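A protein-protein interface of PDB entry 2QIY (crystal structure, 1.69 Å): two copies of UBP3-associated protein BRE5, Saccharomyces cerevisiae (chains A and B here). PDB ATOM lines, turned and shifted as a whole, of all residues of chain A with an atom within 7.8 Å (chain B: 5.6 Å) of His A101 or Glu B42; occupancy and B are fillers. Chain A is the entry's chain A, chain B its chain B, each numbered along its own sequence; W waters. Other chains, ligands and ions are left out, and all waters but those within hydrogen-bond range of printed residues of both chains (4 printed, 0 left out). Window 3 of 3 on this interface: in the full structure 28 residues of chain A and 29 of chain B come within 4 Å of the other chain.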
ATOM      1  N   PHE A  94      -5.802 -14.570  21.962  1.00  0.00           N
ATOM      2  CA  PHE A  94      -4.640 -13.748  21.616  1.00  0.00           C
ATOM      3  C   PHE A  94      -4.957 -12.273  21.621  1.00  0.00           C
ATOM      4  O   PHE A  94      -6.120 -11.869  21.459  1.00  0.00           O
ATOM      5  CB  PHE A  94      -4.063 -14.148  20.254  1.00  0.00           C
ATOM      6  CG  PHE A  94      -5.053 -14.019  19.124  1.00  0.00           C
ATOM      7  CD1 PHE A  94      -5.214 -12.811  18.461  1.00  0.00           C
ATOM      8  CD2 PHE A  94      -5.835 -15.109  18.743  1.00  0.00           C
ATOM      9  CE1 PHE A  94      -6.132 -12.688  17.417  1.00  0.00           C
ATOM     10  CE2 PHE A  94      -6.771 -14.991  17.695  1.00  0.00           C
ATOM     11  CZ  PHE A  94      -6.915 -13.788  17.043  1.00  0.00           C
ATOM     12  N   GLN A  95      -3.899 -11.473  21.783  1.00  0.00           N
ATOM     13  CA  GLN A  95      -3.933 -10.017  21.535  1.00  0.00           C
ATOM     14  C   GLN A  95      -2.580  -9.561  21.008  1.00  0.00           C
ATOM     15  O   GLN A  95      -1.563 -10.214  21.239  1.00  0.00           O
ATOM     16  CB  GLN A  95      -4.228  -9.235  22.820  1.00  0.00           C
ATOM     17  CG  GLN A  95      -5.565  -9.514  23.515  1.00  0.00           C
ATOM     18  CD  GLN A  95      -5.686  -8.791  24.867  1.00  0.00           C
ATOM     19  OE1 GLN A  95      -4.680  -8.366  25.449  1.00  0.00           O
ATOM     20  NE2 GLN A  95      -6.912  -8.650  25.363  1.00  0.00           N
ATOM     21  N   TYR A  96      -2.554  -8.401  20.348  1.00  0.00           N
ATOM     22  CA  TYR A  96      -1.291  -7.776  20.005  1.00  0.00           C
ATOM     23  C   TYR A  96      -0.768  -7.026  21.231  1.00  0.00           C
ATOM     24  O   TYR A  96      -1.547  -6.637  22.105  1.00  0.00           O
ATOM     25  CB  TYR A  96      -1.457  -6.819  18.824  1.00  0.00           C
ATOM     26  CG  TYR A  96      -1.443  -7.505  17.480  1.00  0.00           C
ATOM     27  CD1 TYR A  96      -2.569  -7.495  16.655  1.00  0.00           C
ATOM     28  CD2 TYR A  96      -0.299  -8.169  17.032  1.00  0.00           C
ATOM     29  CE1 TYR A  96      -2.550  -8.129  15.406  1.00  0.00           C
ATOM     30  CE2 TYR A  96      -0.268  -8.800  15.794  1.00  0.00           C
ATOM     31  CZ  TYR A  96      -1.390  -8.782  14.988  1.00  0.00           C
ATOM     32  OH  TYR A  96      -1.339  -9.404  13.752  1.00  0.00           O
ATOM     33  N   THR A  97       0.541  -6.794  21.273  1.00  0.00           N
ATOM     34  CA  THR A  97       1.191  -6.192  22.432  1.00  0.00           C
ATOM     35  C   THR A  97       2.558  -5.638  22.043  1.00  0.00           C
ATOM     36  O   THR A  97       2.973  -5.776  20.897  1.00  0.00           O
ATOM     37  CB  THR A  97       1.362  -7.247  23.560  1.00  0.00           C
ATOM     38  OG1 THR A  97       1.720  -6.593  24.784  1.00  0.00           O
ATOM     39  CG2 THR A  97       2.415  -8.312  23.210  1.00  0.00           C
ATOM     40  N   GLY A  98       3.242  -5.010  22.999  1.00  0.00           N
ATOM     41  CA  GLY A  98       4.643  -4.619  22.816  1.00  0.00           C
ATOM     42  C   GLY A  98       4.868  -3.511  21.804  1.00  0.00           C
ATOM     43  O   GLY A  98       3.928  -2.778  21.415  1.00  0.00           O
ATOM     44  N   HIS A  99       6.120  -3.385  21.375  1.00  0.00           N
ATOM     45  CA  HIS A  99       6.526  -2.287  20.486  1.00  0.00           C
ATOM     46  C   HIS A  99       5.724  -2.271  19.187  1.00  0.00           C
ATOM     47  O   HIS A  99       5.685  -3.274  18.462  1.00  0.00           O
ATOM     48  CB  HIS A  99       8.026  -2.367  20.190  1.00  0.00           C
ATOM     49  CG  HIS A  99       8.544  -1.231  19.359  1.00  0.00           C
ATOM     50  ND1 HIS A  99       9.071  -1.415  18.098  1.00  0.00           N
ATOM     51  CD2 HIS A  99       8.611   0.098  19.605  1.00  0.00           C
ATOM     52  CE1 HIS A  99       9.450  -0.248  17.607  1.00  0.00           C
ATOM     53  NE2 HIS A  99       9.173   0.689  18.497  1.00  0.00           N
ATOM     54  N   LEU A 100       5.079  -1.131  18.926  1.00  0.00           N
ATOM     55  CA  LEU A 100       4.280  -0.894  17.717  1.00  0.00           C
ATOM     56  C   LEU A 100       3.138  -1.903  17.530  1.00  0.00           C
ATOM     57  O   LEU A 100       2.669  -2.114  16.406  1.00  0.00           O
ATOM     58  CB  LEU A 100       5.169  -0.854  16.464  1.00  0.00           C
ATOM     59  CG  LEU A 100       6.209   0.259  16.336  1.00  0.00           C
ATOM     60  CD1 LEU A 100       7.094  -0.004  15.126  1.00  0.00           C
ATOM     61  CD2 LEU A 100       5.532   1.621  16.208  1.00  0.00           C
ATOM     62  N   HIS A 101       2.705  -2.512  18.636  1.00  0.00           N
ATOM     63  CA  HIS A 101       1.634  -3.511  18.644  1.00  0.00           C
ATOM     64  C   HIS A 101       1.916  -4.680  17.684  1.00  0.00           C
ATOM     65  O   HIS A 101       0.990  -5.297  17.177  1.00  0.00           O
ATOM     66  CB  HIS A 101       0.293  -2.830  18.313  1.00  0.00           C
ATOM     67  CG  HIS A 101      -0.862  -3.280  19.160  1.00  0.00           C
ATOM     68  ND1 HIS A 101      -0.747  -3.563  20.506  1.00  0.00           N
ATOM     69  CD2 HIS A 101      -2.175  -3.432  18.858  1.00  0.00           C
ATOM     70  CE1 HIS A 101      -1.932  -3.898  20.989  1.00  0.00           C
ATOM     71  NE2 HIS A 101      -2.816  -3.831  20.008  1.00  0.00           N
ATOM     72  N   LYS A 102       3.199  -4.982  17.454  1.00  0.00           N
ATOM     73  CA  LYS A 102       3.604  -6.035  16.518  1.00  0.00           C
ATOM     74  C   LYS A 102       3.926  -7.395  17.171  1.00  0.00           C
ATOM     75  O   LYS A 102       4.066  -8.408  16.479  1.00  0.00           O
ATOM     76  CB  LYS A 102       4.791  -5.565  15.662  1.00  0.00           C
ATOM     77  CG  LYS A 102       4.468  -4.426  14.683  1.00  0.00           C
ATOM     78  CD  LYS A 102       3.410  -4.846  13.660  1.00  0.00           C
ATOM     79  CE  LYS A 102       3.168  -3.774  12.593  1.00  0.00           C
ATOM     80  NZ  LYS A 102       2.309  -2.627  13.053  1.00  0.00           N
ATOM     81  N   SER A 103       4.063  -7.410  18.490  1.00  0.00           N
ATOM     82  CA  SER A 103       4.237  -8.666  19.223  1.00  0.00           C
ATOM     83  C   SER A 103       2.871  -9.297  19.478  1.00  0.00           C
ATOM     84  O   SER A 103       1.845  -8.612  19.389  1.00  0.00           O
ATOM     85  CB  SER A 103       4.978  -8.410  20.529  1.00  0.00           C
ATOM     86  OG  SER A 103       6.300  -7.977  20.259  1.00  0.00           O
ATOM     87  N   ILE A 104       2.860 -10.598  19.786  1.00  0.00           N
ATOM     88  CA  ILE A 104       1.605 -11.316  19.982  1.00  0.00           C
ATOM     89  C   ILE A 104       1.602 -12.023  21.331  1.00  0.00           C
ATOM     90  O   ILE A 104       2.518 -12.770  21.642  1.00  0.00           O
ATOM     91  CB  ILE A 104       1.350 -12.358  18.861  1.00  0.00           C
ATOM     92  CG1 ILE A 104       1.503 -11.724  17.475  1.00  0.00           C
ATOM     93  CG2 ILE A 104      -0.056 -12.991  19.030  1.00  0.00           C
ATOM     94  CD1 ILE A 104       1.630 -12.733  16.356  1.00  0.00           C
ATOM     95  N   LEU A 105       0.562 -11.761  22.117  1.00  0.00           N
ATOM     96  CA  LEU A 105       0.276 -12.451  23.385  1.00  0.00           C
ATOM     97  C   LEU A 105      -0.674 -13.590  23.094  1.00  0.00           C
ATOM     98  O   LEU A 105      -1.743 -13.361  22.525  1.00  0.00           O
ATOM     99  CB  LEU A 105      -0.446 -11.474  24.328  1.00  0.00           C
ATOM    100  CG  LEU A 105      -0.456 -11.575  25.870  1.00  0.00           C
ATOM    101  CD1 LEU A 105      -1.717 -11.007  26.564  1.00  0.00           C
ATOM    102  CD2 LEU A 105       0.099 -12.858  26.522  1.00  0.00           C
ATOM    103  N   PRO A 130       8.321 -10.203  16.775  1.00  0.00           N
ATOM    104  CA  PRO A 130       8.709 -10.431  15.374  1.00  0.00           C
ATOM    105  C   PRO A 130      10.211 -10.264  15.155  1.00  0.00           C
ATOM    106  O   PRO A 130      10.867  -9.526  15.888  1.00  0.00           O
ATOM    107  CB  PRO A 130       7.930  -9.363  14.596  1.00  0.00           C
ATOM    108  CG  PRO A 130       7.520  -8.328  15.614  1.00  0.00           C
ATOM    109  CD  PRO A 130       7.524  -8.976  16.967  1.00  0.00           C
ATOM    110  N   TYR B  37      -5.510   1.401  32.378  1.00  0.00           N
ATOM    111  CA  TYR B  37      -5.101   0.850  31.085  1.00  0.00           C
ATOM    112  C   TYR B  37      -4.405   1.902  30.206  1.00  0.00           C
ATOM    113  O   TYR B  37      -4.740   3.110  30.243  1.00  0.00           O
ATOM    114  CB  TYR B  37      -6.286   0.282  30.309  1.00  0.00           C
ATOM    115  CG  TYR B  37      -6.959  -0.924  30.925  1.00  0.00           C
ATOM    116  CD1 TYR B  37      -6.777  -2.210  30.390  1.00  0.00           C
ATOM    117  CD2 TYR B  37      -7.807  -0.775  32.030  1.00  0.00           C
ATOM    118  CE1 TYR B  37      -7.425  -3.320  30.944  1.00  0.00           C
ATOM    119  CE2 TYR B  37      -8.451  -1.880  32.604  1.00  0.00           C
ATOM    120  CZ  TYR B  37      -8.249  -3.147  32.062  1.00  0.00           C
ATOM    121  OH  TYR B  37      -8.901  -4.226  32.612  1.00  0.00           O
ATOM    122  N   THR B  40      -4.022   2.599  24.230  1.00  0.00           N
ATOM    123  CA  THR B  40      -4.245   1.631  23.154  1.00  0.00           C
ATOM    124  C   THR B  40      -4.326   0.191  23.680  1.00  0.00           C
ATOM    125  O   THR B  40      -3.975  -0.756  22.957  1.00  0.00           O
ATOM    126  CB  THR B  40      -3.132   1.681  22.088  1.00  0.00           C
ATOM    127  OG1 THR B  40      -1.865   1.403  22.696  1.00  0.00           O
ATOM    128  CG2 THR B  40      -3.086   3.050  21.401  1.00  0.00           C
ATOM    129  N   ALA B  41      -4.762   0.021  24.929  1.00  0.00           N
ATOM    130  CA  ALA B  41      -4.787  -1.323  25.533  1.00  0.00           C
ATOM    131  C   ALA B  41      -5.802  -2.238  24.865  1.00  0.00           C
ATOM    132  O   ALA B  41      -6.757  -1.774  24.262  1.00  0.00           O
ATOM    133  CB  ALA B  41      -5.068  -1.246  27.027  1.00  0.00           C
ATOM    134  N   GLU B  42      -5.551  -3.545  24.964  1.00  0.00           N
ATOM    135  CA  GLU B  42      -6.481  -4.556  24.516  1.00  0.00           C
ATOM    136  C   GLU B  42      -7.038  -5.294  25.724  1.00  0.00           C
ATOM    137  O   GLU B  42      -6.284  -5.750  26.610  1.00  0.00           O
ATOM    138  CB  GLU B  42      -5.802  -5.526  23.554  1.00  0.00           C
ATOM    139  CG  GLU B  42      -5.176  -4.836  22.315  1.00  0.00           C
ATOM    140  CD  GLU B  42      -6.197  -4.446  21.260  1.00  0.00           C
ATOM    141  OE1 GLU B  42      -5.784  -3.811  20.256  1.00  0.00           O
ATOM    142  OE2 GLU B  42      -7.405  -4.765  21.429  1.00  0.00           O
ATOM    143  N   LEU B  43      -8.365  -5.422  25.743  1.00  0.00           N
ATOM    144  CA  LEU B  43      -9.068  -6.148  26.776  1.00  0.00           C
ATOM    145  C   LEU B  43      -9.879  -7.303  26.176  1.00  0.00           C
ATOM    146  O   LEU B  43     -10.523  -7.152  25.118  1.00  0.00           O
ATOM    147  CB  LEU B  43     -10.009  -5.189  27.526  1.00  0.00           C
ATOM    148  CG  LEU B  43     -10.990  -5.765  28.558  1.00  0.00           C
ATOM    149  CD1 LEU B  43     -10.265  -6.356  29.775  1.00  0.00           C
ATOM    150  CD2 LEU B  43     -11.959  -4.647  29.028  1.00  0.00           C
ATOM    151  N   THR B  44      -9.808  -8.458  26.831  1.00  0.00           N
ATOM    152  CA  THR B  44     -10.692  -9.583  26.522  1.00  0.00           C
ATOM    153  C   THR B  44     -11.324 -10.006  27.843  1.00  0.00           C
ATOM    154  O   THR B  44     -10.649 -10.578  28.714  1.00  0.00           O
ATOM    155  CB  THR B  44      -9.913 -10.731  25.869  1.00  0.00           C
ATOM    156  OG1 THR B  44      -9.265 -10.240  24.683  1.00  0.00           O
ATOM    157  CG2 THR B  44     -10.836 -11.927  25.529  1.00  0.00           C
ATOM    158  N   VAL B  65     -12.238  -5.791  23.483  1.00  0.00           N
ATOM    159  CA  VAL B  65     -12.437  -4.342  23.533  1.00  0.00           C
ATOM    160  C   VAL B  65     -11.061  -3.684  23.380  1.00  0.00           C
ATOM    161  O   VAL B  65     -10.108  -4.098  24.034  1.00  0.00           O
ATOM    162  CB  VAL B  65     -13.040  -3.894  24.884  1.00  0.00           C
ATOM    163  CG1 VAL B  65     -13.410  -2.433  24.827  1.00  0.00           C
ATOM    164  CG2 VAL B  65     -14.267  -4.741  25.292  1.00  0.00           C
ATOM    165  N   THR B  66     -10.967  -2.655  22.533  1.00  0.00           N
ATOM    166  CA  THR B  66      -9.698  -2.012  22.211  1.00  0.00           C
ATOM    167  C   THR B  66      -9.717  -0.516  22.501  1.00  0.00           C
ATOM    168  O   THR B  66     -10.640   0.195  22.088  1.00  0.00           O
ATOM    169  CB  THR B  66      -9.367  -2.214  20.712  1.00  0.00           C
ATOM    170  OG1 THR B  66      -9.283  -3.612  20.452  1.00  0.00           O
ATOM    171  CG2 THR B  66      -8.049  -1.559  20.339  1.00  0.00           C
ATOM    172  N   GLY B  67      -8.699  -0.047  23.220  1.00  0.00           N
ATOM    173  CA  GLY B  67      -8.512   1.375  23.495  1.00  0.00           C
ATOM    174  C   GLY B  67      -9.180   1.830  24.785  1.00  0.00           C
ATOM    175  O   GLY B  67     -10.216   1.285  25.162  1.00  0.00           O
ATOM    176  N   ILE B  71     -12.791   0.661  26.471  1.00  0.00           N
ATOM    177  CA  ILE B  71     -12.677  -0.091  27.734  1.00  0.00           C
ATOM    178  C   ILE B  71     -13.498   0.603  28.832  1.00  0.00           C
ATOM    179  O   ILE B  71     -14.212  -0.054  29.600  1.00  0.00           O
ATOM    180  CB  ILE B  71     -11.205  -0.278  28.138  1.00  0.00           C
ATOM    181  CG1 ILE B  71     -10.536  -1.284  27.191  1.00  0.00           C
ATOM    182  CG2 ILE B  71     -11.082  -0.752  29.607  1.00  0.00           C
ATOM    183  CD1 ILE B  71      -9.014  -1.286  27.243  1.00  0.00           C
ATOM    184  N   THR B 140      -1.466  -2.942  29.312  1.00  0.00           N
ATOM    185  CA  THR B 140      -1.572  -2.932  27.855  1.00  0.00           C
ATOM    186  C   THR B 140      -2.403  -4.107  27.336  1.00  0.00           C
ATOM    187  O   THR B 140      -2.951  -4.059  26.222  1.00  0.00           O
ATOM    188  CB  THR B 140      -0.205  -2.947  27.159  1.00  0.00           C
ATOM    189  OG1 THR B 140       0.543  -4.116  27.527  1.00  0.00           O
ATOM    190  CG2 THR B 140       0.570  -1.678  27.517  1.00  0.00           C
ATOM    191  N   ASN B 141      -2.482  -5.153  28.151  1.00  0.00           N
ATOM    192  CA  ASN B 141      -3.186  -6.374  27.784  1.00  0.00           C
ATOM    193  C   ASN B 141      -3.817  -7.003  28.991  1.00  0.00           C
ATOM    194  O   ASN B 141      -3.215  -7.058  30.075  1.00  0.00           O
ATOM    195  CB  ASN B 141      -2.210  -7.399  27.175  1.00  0.00           C
ATOM    196  CG  ASN B 141      -1.583  -6.909  25.894  1.00  0.00           C
ATOM    197  OD1 ASN B 141      -2.072  -7.172  24.788  1.00  0.00           O
ATOM    198  ND2 ASN B 141      -0.511  -6.158  26.028  1.00  0.00           N
ATOM    199  N   ASP B 142      -5.035  -7.499  28.802  1.00  0.00           N
ATOM    200  CA  ASP B 142      -5.762  -8.138  29.875  1.00  0.00           C
ATOM    201  C   ASP B 142      -6.688  -9.146  29.208  1.00  0.00           C
ATOM    202  O   ASP B 142      -7.587  -8.754  28.460  1.00  0.00           O
ATOM    203  CB  ASP B 142      -6.536  -7.028  30.628  1.00  0.00           C
ATOM    204  CG  ASP B 142      -7.536  -7.560  31.661  1.00  0.00           C
ATOM    205  OD1 ASP B 142      -7.756  -8.793  31.768  1.00  0.00           O
ATOM    206  OD2 ASP B 142      -8.103  -6.692  32.376  1.00  0.00           O
ATOM    207  N   ILE B 143      -6.414 -10.436  29.437  1.00  0.00           N
ATOM    208  CA  ILE B 143      -7.234 -11.536  28.853  1.00  0.00           C
ATOM    209  C   ILE B 143      -7.715 -12.447  29.961  1.00  0.00           C
ATOM    210  O   ILE B 143      -6.886 -12.914  30.779  1.00  0.00           O
ATOM    211  CB  ILE B 143      -6.444 -12.418  27.831  1.00  0.00           C
ATOM    212  CG1 ILE B 143      -5.812 -11.600  26.693  1.00  0.00           C
ATOM    213  CG2 ILE B 143      -7.335 -13.565  27.339  1.00  0.00           C
ATOM    214  CD1 ILE B 143      -4.887 -12.404  25.792  1.00  0.00           C
HETATM  215  O   HOH W   1      -4.457  -1.442  20.325  1.00  0.00           O
HETATM  216  O   HOH W   2      -1.815  -3.454  23.746  1.00  0.00           O
HETATM  217  O   HOH W   3      -7.999 -12.371  23.561  1.00  0.00           O
HETATM  218  O   HOH W   4       2.886  -3.651  25.810  1.00  0.00           O
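Of chain B, only Glu B42 (3.0 Å) comes within 4 Å of His A101.
Of the printed residues of chain B, Leu A105 touches Asn B141 (3.7 Å) and Ile B143 (3.5 Å).
Of the printed residues of chain B, Gln A95 touches Glu B42 (3.2 Å), Leu B43 (3.4 Å), Thr B44 (2.9 Å), Asn B141 (2.9 Å), Asp B142 (3.2 Å) and Ile B143 (3.4 Å).
Of the printed residues of chain B, Tyr A96 touches Asn B141.
Gly B67 touches none of the printed residues of chain A.
The nearest residue of chain A that does not touch Glu B42 is Tyr A96 (4.1 Å).
The nearest printed residue of chain A that does not touch Thr B140 is Gln A95 (4.7 Å).
No position is printed for both chains.
Of the 12 pairs that touch across the chains among the printed residues, none has its exchanged pair printed and touching as well.
Water W1 lies within hydrogen-bond range of the side-chain carboxylate (OE1) of Glu B42 (2.7 Å), the backbone carbonyl oxygen (O) of Thr B40 (2.8 Å) and a ring nitrogen (NE2) of His A101 (2.9 Å).
Water W3 bridges OG1 of Thr B44 (2.7 Å) and O of Phe A94 (2.9 Å).
Water W2 bridges the backbone carbonyl oxygen (O) of Thr B140 (2.8 Å) and a ring nitrogen (ND1) of His A101 (3.4 Å).
Water W4 lies within hydrogen-bond range of the side-chain hydroxyl of Thr B140 (2.9 Å), the backbone NH of Gly A98 (3.1 Å) and the side-chain hydroxyl of Thr A97 (3.3 Å).
Along chain A the printed residues that touch a printed residue of chain B span positions 95 to 105.
Of the 14 printed residues of chain B, 7 touch a printed residue of chain A.
Printed residues of chain B that touch a printed residue of chain A: Glu B42, Leu B43, Thr B44, Thr B140, Asn B141, Asp B142 and Ile B143.
Among the printed residues, 12 pairs touch across the chains.
Among the printed residues, no Asp or Glu carboxylate lies within 4 Å of a Lys or Arg side-chain nitrogen of the other chain.
The backbone NH of Leu A105 sits at hydrogen-bond distance from the backbone carbonyl oxygen of Gln A95, 2.8 Å away.
The side-chain hydroxyl (OH) of Tyr B37 sits at hydrogen-bond distance from the side-chain carboxylate (OD2) of Asp B142 (2.6 Å).
O of Thr B140 sits at hydrogen-bond distance from N of Glu B42, 2.9 Å away.
The backbone carbonyl oxygen (O) of Glu B42 is in hydrogen-bond range of the backbone NH (N) of Asp B142 (3.1 Å).
The backbone NH (N) of Val B65 is in hydrogen-bond range of the backbone carbonyl oxygen (O) of Leu B43 (2.7 Å).
N of Thr B44 sits at hydrogen-bond distance from O of Asp B142 (2.8 Å).
The side-chain amide nitrogen (NE2) of Gln A95 is in hydrogen-bond range of the backbone carbonyl oxygen (O) of Glu B42, at 3.2 Å.
The side-chain amide nitrogen (NE2) of Gln A95 is in hydrogen-bond range of the side-chain hydroxyl (OG1) of Thr B44 (2.9 Å).
OD1 of Asn B141 sits close to OE1 of Gln A95, 2.9 Å away.
The backbone carbonyl oxygen (O) of Asp B142 is in hydrogen-bond range of the side-chain amide nitrogen (NE2) of Gln A95, 3.2 Å away.
The backbone carbonyl oxygen (O) of Tyr A96 sits close to the side-chain amide oxygen (OD1) of Asn B141, at 2.8 Å.
The side-chain amide nitrogen (ND2) of Asn B141 lies within hydrogen-bond range of the side-chain hydroxyl (OG1) of Thr A97, 2.6 Å away.
A ring nitrogen (NE2) of His A101 is in hydrogen-bond range of the side-chain carboxylate (OE1) of Glu B42, 3.0 Å away.
Among the printed residues, pairs that only touch across the chains: Gln A95 with Leu B43, Gln A95 with Ile B143, Thr A97 with Thr B140, Leu A105 with Asn B141 and Leu A105 with Ile B143.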
